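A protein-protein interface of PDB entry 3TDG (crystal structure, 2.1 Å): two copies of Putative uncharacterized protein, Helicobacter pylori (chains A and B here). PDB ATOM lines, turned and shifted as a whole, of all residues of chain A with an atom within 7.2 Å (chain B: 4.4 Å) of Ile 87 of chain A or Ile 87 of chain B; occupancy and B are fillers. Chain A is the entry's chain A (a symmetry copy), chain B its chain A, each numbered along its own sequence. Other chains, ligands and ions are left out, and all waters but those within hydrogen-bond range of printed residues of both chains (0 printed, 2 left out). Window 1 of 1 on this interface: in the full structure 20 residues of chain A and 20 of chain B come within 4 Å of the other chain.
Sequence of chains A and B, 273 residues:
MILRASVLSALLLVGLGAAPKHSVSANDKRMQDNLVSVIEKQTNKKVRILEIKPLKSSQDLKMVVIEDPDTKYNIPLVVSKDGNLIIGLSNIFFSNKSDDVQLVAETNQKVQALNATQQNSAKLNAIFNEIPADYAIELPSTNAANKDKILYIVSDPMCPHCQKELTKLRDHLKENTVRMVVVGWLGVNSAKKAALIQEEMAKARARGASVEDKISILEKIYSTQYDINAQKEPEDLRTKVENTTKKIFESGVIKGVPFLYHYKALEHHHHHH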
ATOM      1  N   LEU A  55     -14.362 -13.166  27.422  1.00  0.00           N
ATOM      2  CA  LEU A  55     -13.330 -12.200  27.094  1.00  0.00           C
ATOM      3  C   LEU A  55     -12.284 -12.115  28.189  1.00  0.00           C
ATOM      4  O   LEU A  55     -12.603 -11.993  29.343  1.00  0.00           O
ATOM      5  CB  LEU A  55     -13.915 -10.823  26.894  1.00  0.00           C
ATOM      6  CG  LEU A  55     -14.993 -10.567  25.865  1.00  0.00           C
ATOM      7  CD1 LEU A  55     -15.399  -9.149  25.991  1.00  0.00           C
ATOM      8  CD2 LEU A  55     -14.488 -10.844  24.514  1.00  0.00           C
ATOM      9  N   LEU A  61     -18.392  -9.240  31.025  1.00  0.00           N
ATOM     10  CA  LEU A  61     -18.792  -9.256  29.621  1.00  0.00           C
ATOM     11  C   LEU A  61     -18.429 -10.523  28.859  1.00  0.00           C
ATOM     12  O   LEU A  61     -17.299 -11.004  28.946  1.00  0.00           O
ATOM     13  CB  LEU A  61     -18.209  -8.044  28.911  1.00  0.00           C
ATOM     14  CG  LEU A  61     -18.682  -6.692  29.429  1.00  0.00           C
ATOM     15  CD1 LEU A  61     -18.011  -5.614  28.619  1.00  0.00           C
ATOM     16  CD2 LEU A  61     -20.210  -6.575  29.351  1.00  0.00           C
ATOM     17  N   LYS A  62     -19.399 -11.053  28.111  1.00  0.00           N
ATOM     18  CA  LYS A  62     -19.181 -12.199  27.225  1.00  0.00           C
ATOM     19  C   LYS A  62     -19.451 -11.841  25.755  1.00  0.00           C
ATOM     20  O   LYS A  62     -20.207 -10.918  25.462  1.00  0.00           O
ATOM     21  CB  LYS A  62     -20.072 -13.383  27.627  1.00  0.00           C
ATOM     22  CG  LYS A  62     -20.061 -13.723  29.131  1.00  0.00           C
ATOM     23  CD  LYS A  62     -20.563 -15.139  29.373  1.00  0.00           C
ATOM     24  CE  LYS A  62     -19.434 -16.155  29.223  1.00  0.00           C
ATOM     25  NZ  LYS A  62     -18.506 -16.104  30.398  1.00  0.00           N
ATOM     26  N   VAL A  64     -21.251 -12.881  22.433  1.00  0.00           N
ATOM     27  CA  VAL A  64     -22.399 -13.675  21.989  1.00  0.00           C
ATOM     28  C   VAL A  64     -22.719 -13.384  20.523  1.00  0.00           C
ATOM     29  O   VAL A  64     -22.783 -12.216  20.107  1.00  0.00           O
ATOM     30  CB  VAL A  64     -23.657 -13.384  22.858  1.00  0.00           C
ATOM     31  CG1 VAL A  64     -24.829 -14.276  22.459  1.00  0.00           C
ATOM     32  CG2 VAL A  64     -23.354 -13.577  24.355  1.00  0.00           C
ATOM     33  N   PRO A  76     -22.895 -10.399  15.975  1.00  0.00           N
ATOM     34  CA  PRO A  76     -22.034 -10.483  17.152  1.00  0.00           C
ATOM     35  C   PRO A  76     -22.282  -9.363  18.163  1.00  0.00           C
ATOM     36  O   PRO A  76     -22.450  -8.196  17.797  1.00  0.00           O
ATOM     37  CB  PRO A  76     -20.625 -10.403  16.551  1.00  0.00           C
ATOM     38  CG  PRO A  76     -20.798  -9.536  15.358  1.00  0.00           C
ATOM     39  CD  PRO A  76     -22.151  -9.947  14.786  1.00  0.00           C
ATOM     40  N   LEU A  77     -22.291  -9.746  19.434  1.00  0.00           N
ATOM     41  CA  LEU A  77     -22.623  -8.874  20.558  1.00  0.00           C
ATOM     42  C   LEU A  77     -21.643  -9.042  21.714  1.00  0.00           C
ATOM     43  O   LEU A  77     -21.042 -10.115  21.893  1.00  0.00           O
ATOM     44  CB  LEU A  77     -24.016  -9.250  21.099  1.00  0.00           C
ATOM     45  CG  LEU A  77     -25.173  -9.486  20.109  1.00  0.00           C
ATOM     46  CD1 LEU A  77     -26.382 -10.121  20.825  1.00  0.00           C
ATOM     47  CD2 LEU A  77     -25.552  -8.172  19.434  1.00  0.00           C
ATOM     48  N   VAL A  78     -21.530  -8.002  22.525  1.00  0.00           N
ATOM     49  CA  VAL A  78     -20.981  -8.145  23.878  1.00  0.00           C
ATOM     50  C   VAL A  78     -22.164  -8.022  24.842  1.00  0.00           C
ATOM     51  O   VAL A  78     -22.978  -7.095  24.732  1.00  0.00           O
ATOM     52  CB  VAL A  78     -19.833  -7.118  24.154  1.00  0.00           C
ATOM     53  CG1 VAL A  78     -19.438  -7.108  25.616  1.00  0.00           C
ATOM     54  CG2 VAL A  78     -18.609  -7.481  23.310  1.00  0.00           C
ATOM     55  N   VAL A  79     -22.276  -8.984  25.750  1.00  0.00           N
ATOM     56  CA  VAL A  79     -23.428  -9.097  26.642  1.00  0.00           C
ATOM     57  C   VAL A  79     -22.969  -9.258  28.104  1.00  0.00           C
ATOM     58  O   VAL A  79     -22.034 -10.013  28.389  1.00  0.00           O
ATOM     59  CB  VAL A  79     -24.341 -10.285  26.215  1.00  0.00           C
ATOM     60  CG1 VAL A  79     -25.507 -10.470  27.171  1.00  0.00           C
ATOM     61  CG2 VAL A  79     -24.860 -10.105  24.779  1.00  0.00           C
ATOM     62  N   SER A  80     -23.613  -8.541  29.023  1.00  0.00           N
ATOM     63  CA  SER A  80     -23.331  -8.712  30.455  1.00  0.00           C
ATOM     64  C   SER A  80     -23.751 -10.102  30.961  1.00  0.00           C
ATOM     65  O   SER A  80     -24.514 -10.816  30.291  1.00  0.00           O
ATOM     66  CB  SER A  80     -23.983  -7.606  31.290  1.00  0.00           C
ATOM     67  OG  SER A  80     -25.394  -7.627  31.157  1.00  0.00           O
ATOM     68  N   LEU A  85     -27.496  -6.069  29.499  1.00  0.00           N
ATOM     69  CA  LEU A  85     -26.823  -5.063  28.678  1.00  0.00           C
ATOM     70  C   LEU A  85     -26.247  -5.756  27.441  1.00  0.00           C
ATOM     71  O   LEU A  85     -25.583  -6.788  27.531  1.00  0.00           O
ATOM     72  CB  LEU A  85     -25.729  -4.340  29.480  1.00  0.00           C
ATOM     73  CG  LEU A  85     -24.787  -3.367  28.746  1.00  0.00           C
ATOM     74  CD1 LEU A  85     -25.528  -2.143  28.193  1.00  0.00           C
ATOM     75  CD2 LEU A  85     -23.661  -2.949  29.673  1.00  0.00           C
ATOM     76  N   ILE A  86     -26.546  -5.197  26.275  1.00  0.00           N
ATOM     77  CA  ILE A  86     -26.253  -5.842  25.018  1.00  0.00           C
ATOM     78  C   ILE A  86     -25.718  -4.759  24.098  1.00  0.00           C
ATOM     79  O   ILE A  86     -26.403  -3.759  23.836  1.00  0.00           O
ATOM     80  CB  ILE A  86     -27.536  -6.490  24.426  1.00  0.00           C
ATOM     81  CG1 ILE A  86     -27.985  -7.686  25.276  1.00  0.00           C
ATOM     82  CG2 ILE A  86     -27.323  -6.926  22.979  1.00  0.00           C
ATOM     83  CD1 ILE A  86     -29.480  -7.837  25.446  1.00  0.00           C
ATOM     84  N   ILE A  87     -24.494  -4.960  23.612  1.00  0.00           N
ATOM     85  CA  ILE A  87     -23.828  -3.997  22.744  1.00  0.00           C
ATOM     86  C   ILE A  87     -23.391  -4.723  21.479  1.00  0.00           C
ATOM     87  O   ILE A  87     -22.733  -5.765  21.557  1.00  0.00           O
ATOM     88  CB  ILE A  87     -22.602  -3.361  23.449  1.00  0.00           C
ATOM     89  CG1 ILE A  87     -23.046  -2.681  24.741  1.00  0.00           C
ATOM     90  CG2 ILE A  87     -21.905  -2.332  22.532  1.00  0.00           C
ATOM     91  CD1 ILE A  87     -21.942  -2.515  25.781  1.00  0.00           C
ATOM     92  N   GLY A  88     -23.766  -4.190  20.313  1.00  0.00           N
ATOM     93  CA  GLY A  88     -23.340  -4.796  19.052  1.00  0.00           C
ATOM     94  C   GLY A  88     -21.830  -4.648  18.850  1.00  0.00           C
ATOM     95  O   GLY A  88     -21.273  -3.573  19.104  1.00  0.00           O
ATOM     96  N   LEU A  89     -21.174  -5.718  18.406  1.00  0.00           N
ATOM     97  CA  LEU A  89     -19.746  -5.670  18.071  1.00  0.00           C
ATOM     98  C   LEU A  89     -19.549  -5.161  16.658  1.00  0.00           C
ATOM     99  O   LEU A  89     -20.404  -5.345  15.796  1.00  0.00           O
ATOM    100  CB  LEU A  89     -19.094  -7.046  18.193  1.00  0.00           C
ATOM    101  CG  LEU A  89     -18.514  -7.489  19.539  1.00  0.00           C
ATOM    102  CD1 LEU A  89     -18.022  -8.908  19.442  1.00  0.00           C
ATOM    103  CD2 LEU A  89     -17.383  -6.556  19.971  1.00  0.00           C
ATOM    104  N   SER A  90     -18.409  -4.518  16.434  1.00  0.00           N
ATOM    105  CA  SER A  90     -18.055  -3.972  15.134  1.00  0.00           C
ATOM    106  C   SER A  90     -16.538  -3.981  15.043  1.00  0.00           C
ATOM    107  O   SER A  90     -15.875  -4.512  15.935  1.00  0.00           O
ATOM    108  CB  SER A  90     -18.577  -2.535  15.009  1.00  0.00           C
ATOM    109  OG  SER A  90     -17.817  -1.639  15.818  1.00  0.00           O
ATOM    110  N   ILE A  92     -14.873  -1.326  15.489  1.00  0.00           N
ATOM    111  CA  ILE A  92     -14.424  -0.453  16.573  1.00  0.00           C
ATOM    112  C   ILE A  92     -14.417  -1.272  17.852  1.00  0.00           C
ATOM    113  O   ILE A  92     -15.403  -1.312  18.596  1.00  0.00           O
ATOM    114  CB  ILE A  92     -15.260   0.835  16.694  1.00  0.00           C
ATOM    115  CG1 ILE A  92     -15.292   1.563  15.348  1.00  0.00           C
ATOM    116  CG2 ILE A  92     -14.710   1.764  17.833  1.00  0.00           C
ATOM    117  CD1 ILE A  92     -16.352   2.660  15.242  1.00  0.00           C
ATOM    118  N   PHE A  93     -13.293  -1.962  18.058  1.00  0.00           N
ATOM    119  CA  PHE A  93     -13.049  -2.801  19.211  1.00  0.00           C
ATOM    120  C   PHE A  93     -11.552  -2.761  19.556  1.00  0.00           C
ATOM    121  O   PHE A  93     -10.705  -3.090  18.727  1.00  0.00           O
ATOM    122  CB  PHE A  93     -13.434  -4.256  18.937  1.00  0.00           C
ATOM    123  CG  PHE A  93     -13.183  -5.151  20.101  1.00  0.00           C
ATOM    124  CD1 PHE A  93     -14.161  -5.321  21.085  1.00  0.00           C
ATOM    125  CD2 PHE A  93     -11.952  -5.782  20.261  1.00  0.00           C
ATOM    126  CE1 PHE A  93     -13.925  -6.114  22.196  1.00  0.00           C
ATOM    127  CE2 PHE A  93     -11.699  -6.582  21.382  1.00  0.00           C
ATOM    128  CZ  PHE A  93     -12.688  -6.744  22.348  1.00  0.00           C
ATOM    129  N   PHE A  94     -11.224  -2.378  20.774  1.00  0.00           N
ATOM    130  CA  PHE A  94      -9.816  -2.363  21.182  1.00  0.00           C
ATOM    131  C   PHE A  94      -9.686  -2.930  22.555  1.00  0.00           C
ATOM    132  O   PHE A  94     -10.568  -2.757  23.408  1.00  0.00           O
ATOM    133  CB  PHE A  94      -9.212  -0.962  21.114  1.00  0.00           C
ATOM    134  CG  PHE A  94      -9.460  -0.275  19.809  1.00  0.00           C
ATOM    135  CD1 PHE A  94      -8.674  -0.567  18.694  1.00  0.00           C
ATOM    136  CD2 PHE A  94     -10.493   0.637  19.682  1.00  0.00           C
ATOM    137  CE1 PHE A  94      -8.924   0.042  17.471  1.00  0.00           C
ATOM    138  CE2 PHE A  94     -10.745   1.258  18.463  1.00  0.00           C
ATOM    139  CZ  PHE A  94      -9.960   0.963  17.358  1.00  0.00           C
ATOM    140  N   LEU B  61     -18.645  -0.585  33.175  1.00  0.00           N
ATOM    141  CA  LEU B  61     -18.670   0.089  31.880  1.00  0.00           C
ATOM    142  C   LEU B  61     -19.148   1.533  31.912  1.00  0.00           C
ATOM    143  O   LEU B  61     -20.167   1.843  32.530  1.00  0.00           O
ATOM    144  CB  LEU B  61     -19.519  -0.713  30.905  1.00  0.00           C
ATOM    145  CG  LEU B  61     -19.013  -2.116  30.597  1.00  0.00           C
ATOM    146  CD1 LEU B  61     -19.965  -2.760  29.623  1.00  0.00           C
ATOM    147  CD2 LEU B  61     -17.586  -2.077  30.034  1.00  0.00           C
ATOM    148  N   LEU B  77     -18.257   5.355  22.480  1.00  0.00           N
ATOM    149  CA  LEU B  77     -17.676   4.095  22.940  1.00  0.00           C
ATOM    150  C   LEU B  77     -18.263   3.656  24.277  1.00  0.00           C
ATOM    151  O   LEU B  77     -18.708   4.487  25.085  1.00  0.00           O
ATOM    152  CB  LEU B  77     -16.162   4.286  23.162  1.00  0.00           C
ATOM    153  CG  LEU B  77     -15.329   5.022  22.096  1.00  0.00           C
ATOM    154  CD1 LEU B  77     -13.922   5.353  22.634  1.00  0.00           C
ATOM    155  CD2 LEU B  77     -15.257   4.183  20.825  1.00  0.00           C
ATOM    156  N   VAL B  78     -18.209   2.357  24.528  1.00  0.00           N
ATOM    157  CA  VAL B  78     -18.329   1.837  25.894  1.00  0.00           C
ATOM    158  C   VAL B  78     -16.929   1.378  26.308  1.00  0.00           C
ATOM    159  O   VAL B  78     -16.250   0.659  25.563  1.00  0.00           O
ATOM    160  CB  VAL B  78     -19.417   0.717  25.999  1.00  0.00           C
ATOM    161  CG1 VAL B  78     -19.370   0.022  27.343  1.00  0.00           C
ATOM    162  CG2 VAL B  78     -20.805   1.333  25.806  1.00  0.00           C
ATOM    163  N   LEU B  85     -10.626  -2.078  27.814  1.00  0.00           N
ATOM    164  CA  LEU B  85     -11.578  -2.652  26.864  1.00  0.00           C
ATOM    165  C   LEU B  85     -12.438  -1.519  26.298  1.00  0.00           C
ATOM    166  O   LEU B  85     -12.972  -0.688  27.031  1.00  0.00           O
ATOM    167  CB  LEU B  85     -12.440  -3.734  27.534  1.00  0.00           C
ATOM    168  CG  LEU B  85     -13.622  -4.337  26.751  1.00  0.00           C
ATOM    169  CD1 LEU B  85     -13.161  -5.125  25.518  1.00  0.00           C
ATOM    170  CD2 LEU B  85     -14.456  -5.205  27.673  1.00  0.00           C
ATOM    171  N   ILE B  86     -12.531  -1.472  24.976  1.00  0.00           N
ATOM    172  CA  ILE B  86     -13.130  -0.353  24.290  1.00  0.00           C
ATOM    173  C   ILE B  86     -13.985  -0.941  23.180  1.00  0.00           C
ATOM    174  O   ILE B  86     -13.478  -1.665  22.310  1.00  0.00           O
ATOM    175  CB  ILE B  86     -12.032   0.581  23.708  1.00  0.00           C
ATOM    176  CG1 ILE B  86     -11.272   1.296  24.833  1.00  0.00           C
ATOM    177  CG2 ILE B  86     -12.625   1.605  22.744  1.00  0.00           C
ATOM    178  CD1 ILE B  86      -9.785   1.460  24.610  1.00  0.00           C
ATOM    179  N   ILE B  87     -15.280  -0.630  23.216  1.00  0.00           N
ATOM    180  CA  ILE B  87     -16.236  -1.144  22.243  1.00  0.00           C
ATOM    181  C   ILE B  87     -16.969   0.039  21.629  1.00  0.00           C
ATOM    182  O   ILE B  87     -17.501   0.886  22.354  1.00  0.00           O
ATOM    183  CB  ILE B  87     -17.246  -2.114  22.909  1.00  0.00           C
ATOM    184  CG1 ILE B  87     -16.495  -3.270  23.565  1.00  0.00           C
ATOM    185  CG2 ILE B  87     -18.250  -2.668  21.875  1.00  0.00           C
ATOM    186  CD1 ILE B  87     -17.258  -3.964  24.691  1.00  0.00           C
ATOM    187  N   GLY B  88     -16.988   0.116  20.295  1.00  0.00           N
ATOM    188  CA  GLY B  88     -17.718   1.192  19.626  1.00  0.00           C
ATOM    189  C   GLY B  88     -19.228   1.045  19.827  1.00  0.00           C
ATOM    190  O   GLY B  88     -19.762  -0.066  19.720  1.00  0.00           O
ATOM    191  N   LEU B  89     -19.907   2.150  20.125  1.00  0.00           N
ATOM    192  CA  LEU B  89     -21.371   2.158  20.235  1.00  0.00           C
ATOM    193  C   LEU B  89     -22.004   2.326  18.870  1.00  0.00           C
ATOM    194  O   LEU B  89     -21.426   2.938  17.976  1.00  0.00           O
ATOM    195  CB  LEU B  89     -21.859   3.281  21.147  1.00  0.00           C
ATOM    196  CG  LEU B  89     -21.991   3.030  22.652  1.00  0.00           C
ATOM    197  CD1 LEU B  89     -22.387   4.301  23.351  1.00  0.00           C
ATOM    198  CD2 LEU B  89     -23.010   1.924  22.925  1.00  0.00           C
ATOM    199  N   ILE B  92     -27.079  -0.894  17.517  1.00  0.00           N
ATOM    200  CA  ILE B  92     -27.253  -2.191  18.171  1.00  0.00           C
ATOM    201  C   ILE B  92     -26.831  -2.037  19.622  1.00  0.00           C
ATOM    202  O   ILE B  92     -25.670  -2.266  19.981  1.00  0.00           O
ATOM    203  CB  ILE B  92     -26.512  -3.333  17.450  1.00  0.00           C
ATOM    204  CG1 ILE B  92     -26.925  -3.373  15.977  1.00  0.00           C
ATOM    205  CG2 ILE B  92     -26.772  -4.712  18.155  1.00  0.00           C
ATOM    206  CD1 ILE B  92     -26.021  -4.228  15.086  1.00  0.00           C
ATOM    207  N   PHE B  93     -27.794  -1.595  20.432  1.00  0.00           N
ATOM    208  CA  PHE B  93     -27.632  -1.384  21.853  1.00  0.00           C
ATOM    209  C   PHE B  93     -28.963  -1.681  22.562  1.00  0.00           C
ATOM    210  O   PHE B  93     -29.990  -1.075  22.256  1.00  0.00           O
ATOM    211  CB  PHE B  93     -27.242   0.062  22.164  1.00  0.00           C
ATOM    212  CG  PHE B  93     -27.080   0.317  23.624  1.00  0.00           C
ATOM    213  CD1 PHE B  93     -25.849   0.095  24.247  1.00  0.00           C
ATOM    214  CD2 PHE B  93     -28.163   0.721  24.400  1.00  0.00           C
ATOM    215  CE1 PHE B  93     -25.694   0.286  25.610  1.00  0.00           C
ATOM    216  CE2 PHE B  93     -28.022   0.910  25.779  1.00  0.00           C
ATOM    217  CZ  PHE B  93     -26.787   0.690  26.381  1.00  0.00           C
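O of Ile 86 of chain B is in hydrogen-bond range of N of Phe 94 of chain A, at 2.8 Å. The backbone NH (N) of Gly 88 of chain B is in hydrogen-bond range of the backbone carbonyl oxygen (O) of Ile 92 of chain A (2.7 Å). O of Ile 92 of chain B lies within hydrogen-bond range of N of Gly 88 of chain A.
O of Ile 87 of chain B sits at hydrogen-bond distance from N of Val 78 of chain B (2.7 Å). The backbone NH (N) of Leu 77 of chain A lies within hydrogen-bond range of the backbone carbonyl oxygen (O) of Val 64 of chain A, at 2.6 Å. N of Val 78 of chain A sits at hydrogen-bond distance from O of Ile 87 of chain A, 2.7 Å away. N of Ser 80 of chain A sits at hydrogen-bond distance from O of Leu 85 of chain A (3.0 Å). The side-chain hydroxyl of Ser 90 of chain A lies within hydrogen-bond range of the backbone NH of Ile 92 of chain A, 3.0 Å away.
Leu 77 of chain A touches Ile 92 of chain B. Val 78 of chain A touches Ile 87 of chain B. CD1 of Leu 85 of chain A touches CE1 of Phe 93 of chain B (3.5 Å). Phe 93 of chain B touches Ile 86 of chain A. CG2 of Ile 87 of chain A touches CG2 of Ile 87 of chain B, at 3.7 Å. Ile 92 of chain B touches Ile 87 of chain A. Phe 93 of chain B touches Ile 87 of chain A. O of Gly 88 of chain B touches O of Gly 88 of chain A, at 3.9 Å. Ile 92 of chain A touches Leu 77 of chain B. CD1 of Phe 93 of chain A touches CG1 of Ile 87 of chain B, 3.98 Å away.
Val 64 of chain A touches none of the printed residues of chain B. Ile 87 of chain A touches just these residues of chain B: Val 78 (3.9 Å), Ile 87 (3.7 Å), Ile 92 (3.7 Å) and Phe 93 (3.98 Å). Of the printed residues of chain B, Gly 88 of chain A touches Gly 88 and Ile 92. Of the printed residues of chain B, Phe 93 of chain A touches Leu 85, Ile 86 and Ile 87. Of the printed residues of chain A, Leu 61 of chain B touches Leu 61 and Leu 85. Ile 87 of chain B touches just these residues of chain A: Val 78, Ile 87, Ile 92 and Phe 93. The nearest residue of chain B that does not touch Ile 87 of chain A is Gly 88 of chain B (4.2 Å). The nearest printed residue of chain B that does not touch Val 78 of chain A is Leu 85 of chain B (5.7 Å).
Hydrophobic or aromatic side chains of chain A that line the printed part of chain B: Leu 61, Leu 77, Val 78, Leu 85, Ile 87, Ile 92, Phe 93 and Phe 94. Of the 10 printed residues of chain B, 9 touch a printed residue of chain A. Hydrophobic or aromatic side chains of chain B within 4 Å of the printed part of chain A: Leu 61, Leu 77, Val 78, Leu 85, Ile 86, Ile 87, Ile 92 and Phe 93. Among the printed residues, 21 pairs touch across the chains.
Leu 61 of chain A touches its own counterpart, Leu 61 of chain B. Leu 61 of chain A touches Leu 85 of chain B, and with the chains exchanged Leu 85 of chain A touches Leu 61 of chain B. Leu 85 of chain A touches Phe 93 of chain B, and with the chains exchanged Phe 93 of chain A touches Leu 85 of chain B. Gly 88 of chain A touches its own counterpart, Gly 88 of chain B.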
